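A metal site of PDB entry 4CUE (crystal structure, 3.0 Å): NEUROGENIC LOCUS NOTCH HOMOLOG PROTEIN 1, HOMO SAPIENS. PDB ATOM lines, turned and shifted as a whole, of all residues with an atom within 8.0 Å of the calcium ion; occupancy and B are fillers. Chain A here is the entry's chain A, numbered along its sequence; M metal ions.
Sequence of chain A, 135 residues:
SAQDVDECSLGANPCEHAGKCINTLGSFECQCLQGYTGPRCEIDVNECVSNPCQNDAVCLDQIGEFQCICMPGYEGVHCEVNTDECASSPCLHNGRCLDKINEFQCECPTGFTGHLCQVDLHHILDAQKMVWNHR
The backbone NH (N) of Val 45 is in hydrogen-bond range of the backbone carbonyl oxygen (O) of Gly 35 (2.9 Å).
OD2 of Asp 61 sits close to OD1 of Asn 46 (3.3 Å).
The side-chain sulfur (SG) of Cys 48 sits at hydrogen-bond distance from the backbone NH (N) of Asp 61, at 3.6 Å.
Five residues have an atom within 4 Å of the calcium ion: Asp 44, Val 45, Glu 47, Asp 61 and Gln 62.
The nearest printed residue that does not touch the calcium ion is Ile 63 (4.2 Å).
The calcium ion is bound by the backbone carbonyl oxygen of Gln 62 (2.2 Å), the backbone carbonyl oxygen of Val 45 (2.3 Å), the side-chain carboxylate of Asp 44 (2.4 Å), the side-chain carboxylate of Asp 61 (2.4 Å) and the side-chain carboxylate of Glu 47 (2.4 Å).
The calcium ion has five donor atoms within binding distance.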
ATOM      1  N   GLN A  34      29.631  19.270   7.392  1.00  0.00           N
ATOM      2  CA  GLN A  34      28.626  19.811   8.307  1.00  0.00           C
ATOM      3  C   GLN A  34      28.253  21.230   7.945  1.00  0.00           C
ATOM      4  O   GLN A  34      29.122  22.081   7.729  1.00  0.00           O
ATOM      5  CB  GLN A  34      29.094  19.706   9.759  1.00  0.00           C
ATOM      6  CG  GLN A  34      27.945  19.895  10.755  1.00  0.00           C
ATOM      7  CD  GLN A  34      28.154  19.170  12.068  1.00  0.00           C
ATOM      8  OE1 GLN A  34      28.821  18.130  12.153  1.00  0.00           O
ATOM      9  NE2 GLN A  34      27.537  19.679  13.130  1.00  0.00           N
ATOM     10  N   GLY A  35      26.961  21.442   7.828  1.00  0.00           N
ATOM     11  CA  GLY A  35      26.411  22.745   7.474  1.00  0.00           C
ATOM     12  C   GLY A  35      26.026  22.886   6.017  1.00  0.00           C
ATOM     13  O   GLY A  35      25.473  23.923   5.630  1.00  0.00           O
ATOM     14  N   TYR A  36      26.302  21.846   5.186  1.00  0.00           N
ATOM     15  CA  TYR A  36      25.964  21.890   3.770  1.00  0.00           C
ATOM     16  C   TYR A  36      25.057  20.766   3.305  1.00  0.00           C
ATOM     17  O   TYR A  36      25.120  19.653   3.833  1.00  0.00           O
ATOM     18  CB  TYR A  36      27.217  21.969   2.917  1.00  0.00           C
ATOM     19  CG  TYR A  36      28.081  23.158   3.252  1.00  0.00           C
ATOM     20  CD1 TYR A  36      27.764  24.439   2.774  1.00  0.00           C
ATOM     21  CD2 TYR A  36      29.238  23.010   4.031  1.00  0.00           C
ATOM     22  CE1 TYR A  36      28.577  25.536   3.063  1.00  0.00           C
ATOM     23  CE2 TYR A  36      30.064  24.092   4.309  1.00  0.00           C
ATOM     24  CZ  TYR A  36      29.746  25.355   3.817  1.00  0.00           C
ATOM     25  OH  TYR A  36      30.629  26.385   4.086  1.00  0.00           O
ATOM     26  N   ILE A  43      24.024  24.028  -1.061  1.00  0.00           N
ATOM     27  CA  ILE A  43      23.313  24.814  -0.069  1.00  0.00           C
ATOM     28  C   ILE A  43      23.943  24.949   1.293  1.00  0.00           C
ATOM     29  O   ILE A  43      24.256  23.958   1.946  1.00  0.00           O
ATOM     30  CB  ILE A  43      21.847  24.368   0.050  1.00  0.00           C
ATOM     31  CG1 ILE A  43      21.213  24.174  -1.338  1.00  0.00           C
ATOM     32  CG2 ILE A  43      21.033  25.354   0.917  1.00  0.00           C
ATOM     33  CD1 ILE A  43      19.915  23.371  -1.331  1.00  0.00           C
ATOM     34  N   ASP A  44      24.036  26.191   1.748  1.00  0.00           N
ATOM     35  CA  ASP A  44      24.470  26.514   3.083  1.00  0.00           C
ATOM     36  C   ASP A  44      23.198  26.443   3.949  1.00  0.00           C
ATOM     37  O   ASP A  44      22.343  27.328   3.892  1.00  0.00           O
ATOM     38  CB  ASP A  44      25.079  27.924   3.067  1.00  0.00           C
ATOM     39  CG  ASP A  44      25.272  28.578   4.404  1.00  0.00           C
ATOM     40  OD1 ASP A  44      25.047  27.897   5.435  1.00  0.00           O
ATOM     41  OD2 ASP A  44      25.662  29.774   4.442  1.00  0.00           O
ATOM     42  N   VAL A  45      23.074  25.370   4.742  1.00  0.00           N
ATOM     43  CA  VAL A  45      21.945  25.163   5.659  1.00  0.00           C
ATOM     44  C   VAL A  45      21.746  26.401   6.554  1.00  0.00           C
ATOM     45  O   VAL A  45      22.719  26.996   7.027  1.00  0.00           O
ATOM     46  CB  VAL A  45      22.132  23.908   6.555  1.00  0.00           C
ATOM     47  CG1 VAL A  45      20.996  23.738   7.568  1.00  0.00           C
ATOM     48  CG2 VAL A  45      22.255  22.658   5.713  1.00  0.00           C
ATOM     49  N   ASN A  46      20.477  26.756   6.788  1.00  0.00           N
ATOM     50  CA  ASN A  46      20.114  27.839   7.696  1.00  0.00           C
ATOM     51  C   ASN A  46      19.898  27.221   9.085  1.00  0.00           C
ATOM     52  O   ASN A  46      18.809  26.703   9.371  1.00  0.00           O
ATOM     53  CB  ASN A  46      18.840  28.592   7.226  1.00  0.00           C
ATOM     54  CG  ASN A  46      18.365  29.655   8.192  1.00  0.00           C
ATOM     55  OD1 ASN A  46      19.068  30.066   9.113  1.00  0.00           O
ATOM     56  ND2 ASN A  46      17.139  30.126   8.000  1.00  0.00           N
ATOM     57  N   GLU A  47      20.912  27.275   9.945  1.00  0.00           N
ATOM     58  CA  GLU A  47      20.832  26.717  11.297  1.00  0.00           C
ATOM     59  C   GLU A  47      19.874  27.451  12.219  1.00  0.00           C
ATOM     60  O   GLU A  47      19.606  26.966  13.323  1.00  0.00           O
ATOM     61  CB  GLU A  47      22.216  26.628  11.936  1.00  0.00           C
ATOM     62  CG  GLU A  47      23.024  25.459  11.426  1.00  0.00           C
ATOM     63  CD  GLU A  47      23.721  25.713  10.116  1.00  0.00           C
ATOM     64  OE1 GLU A  47      23.745  26.867   9.655  1.00  0.00           O
ATOM     65  OE2 GLU A  47      24.232  24.736   9.528  1.00  0.00           O
ATOM     66  N   CYS A  48      19.321  28.591  11.768  1.00  0.00           N
ATOM     67  CA  CYS A  48      18.368  29.426  12.507  1.00  0.00           C
ATOM     68  C   CYS A  48      16.913  29.113  12.166  1.00  0.00           C
ATOM     69  O   CYS A  48      16.001  29.641  12.815  1.00  0.00           O
ATOM     70  CB  CYS A  48      18.695  30.893  12.280  1.00  0.00           C
ATOM     71  SG  CYS A  48      20.319  31.365  12.904  1.00  0.00           S
ATOM     72  N   LEU A  60      22.422  34.091  14.467  1.00  0.00           N
ATOM     73  CA  LEU A  60      23.404  34.223  13.384  1.00  0.00           C
ATOM     74  C   LEU A  60      23.570  32.878  12.704  1.00  0.00           C
ATOM     75  O   LEU A  60      23.987  31.910  13.331  1.00  0.00           O
ATOM     76  CB  LEU A  60      24.765  34.719  13.874  1.00  0.00           C
ATOM     77  CG  LEU A  60      24.799  35.998  14.680  1.00  0.00           C
ATOM     78  CD1 LEU A  60      26.204  36.261  15.157  1.00  0.00           C
ATOM     79  CD2 LEU A  60      24.203  37.179  13.892  1.00  0.00           C
ATOM     80  N   ASP A  61      23.220  32.838  11.421  1.00  0.00           N
ATOM     81  CA  ASP A  61      23.318  31.665  10.584  1.00  0.00           C
ATOM     82  C   ASP A  61      24.742  31.567   9.988  1.00  0.00           C
ATOM     83  O   ASP A  61      25.114  32.312   9.094  1.00  0.00           O
ATOM     84  CB  ASP A  61      22.222  31.728   9.523  1.00  0.00           C
ATOM     85  CG  ASP A  61      22.323  30.658   8.452  1.00  0.00           C
ATOM     86  OD1 ASP A  61      22.992  29.621   8.684  1.00  0.00           O
ATOM     87  OD2 ASP A  61      21.733  30.844   7.361  1.00  0.00           O
ATOM     88  N   GLN A  62      25.533  30.660  10.541  1.00  0.00           N
ATOM     89  CA  GLN A  62      26.942  30.491  10.204  1.00  0.00           C
ATOM     90  C   GLN A  62      27.218  29.146   9.526  1.00  0.00           C
ATOM     91  O   GLN A  62      26.282  28.420   9.172  1.00  0.00           O
ATOM     92  CB  GLN A  62      27.794  30.683  11.450  1.00  0.00           C
ATOM     93  CG  GLN A  62      27.475  31.970  12.173  1.00  0.00           C
ATOM     94  CD  GLN A  62      28.101  32.044  13.546  1.00  0.00           C
ATOM     95  OE1 GLN A  62      28.461  31.012  14.157  1.00  0.00           O
ATOM     96  NE2 GLN A  62      28.230  33.270  14.051  1.00  0.00           N
ATOM     97  N   ILE A  63      28.484  28.825   9.307  1.00  0.00           N
ATOM     98  CA  ILE A  63      28.795  27.601   8.591  1.00  0.00           C
ATOM     99  C   ILE A  63      28.743  26.451   9.557  1.00  0.00           C
ATOM    100  O   ILE A  63      29.612  26.367  10.438  1.00  0.00           O
ATOM    101  CB  ILE A  63      30.158  27.730   7.857  1.00  0.00           C
ATOM    102  CG1 ILE A  63      30.163  28.879   6.801  1.00  0.00           C
ATOM    103  CG2 ILE A  63      30.602  26.384   7.252  1.00  0.00           C
ATOM    104  CD1 ILE A  63      30.800  30.305   7.265  1.00  0.00           C
ATOM    105  N   GLY A  64      27.727  25.601   9.411  1.00  0.00           N
ATOM    106  CA  GLY A  64      27.552  24.428  10.261  1.00  0.00           C
ATOM    107  C   GLY A  64      27.155  24.714  11.700  1.00  0.00           C
ATOM    108  O   GLY A  64      27.258  23.837  12.578  1.00  0.00           O
ATOM    109  N   GLU A  65      26.687  25.935  11.969  1.00  0.00           N
ATOM    110  CA  GLU A  65      26.302  26.315  13.304  1.00  0.00           C
ATOM    111  C   GLU A  65      25.511  27.626  13.314  1.00  0.00           C
ATOM    112  O   GLU A  65      25.450  28.380  12.332  1.00  0.00           O
ATOM    113  CB  GLU A  65      27.546  26.424  14.238  1.00  0.00           C
ATOM    114  CG  GLU A  65      28.515  27.561  13.906  1.00  0.00           C
ATOM    115  CD  GLU A  65      29.779  27.582  14.741  1.00  0.00           C
ATOM    116  OE1 GLU A  65      29.674  27.796  15.974  1.00  0.00           O
ATOM    117  OE2 GLU A  65      30.868  27.398  14.164  1.00  0.00           O
ATOM    118  N   PHE A  66      24.922  27.879  14.459  1.00  0.00           N
ATOM    119  CA  PHE A  66      24.294  29.147  14.738  1.00  0.00           C
ATOM    120  C   PHE A  66      24.967  29.708  15.974  1.00  0.00           C
ATOM    121  O   PHE A  66      25.575  28.956  16.733  1.00  0.00           O
ATOM    122  CB  PHE A  66      22.776  29.029  14.942  1.00  0.00           C
ATOM    123  CG  PHE A  66      22.402  28.204  16.144  1.00  0.00           C
ATOM    124  CD1 PHE A  66      22.276  26.832  16.053  1.00  0.00           C
ATOM    125  CD2 PHE A  66      22.232  28.800  17.375  1.00  0.00           C
ATOM    126  CE1 PHE A  66      21.975  26.066  17.170  1.00  0.00           C
ATOM    127  CE2 PHE A  66      21.961  28.035  18.490  1.00  0.00           C
ATOM    128  CZ  PHE A  66      21.807  26.681  18.377  1.00  0.00           C
HETATM  129 CA    CA M   1      24.615  28.116   7.740  1.00  0.00          CA
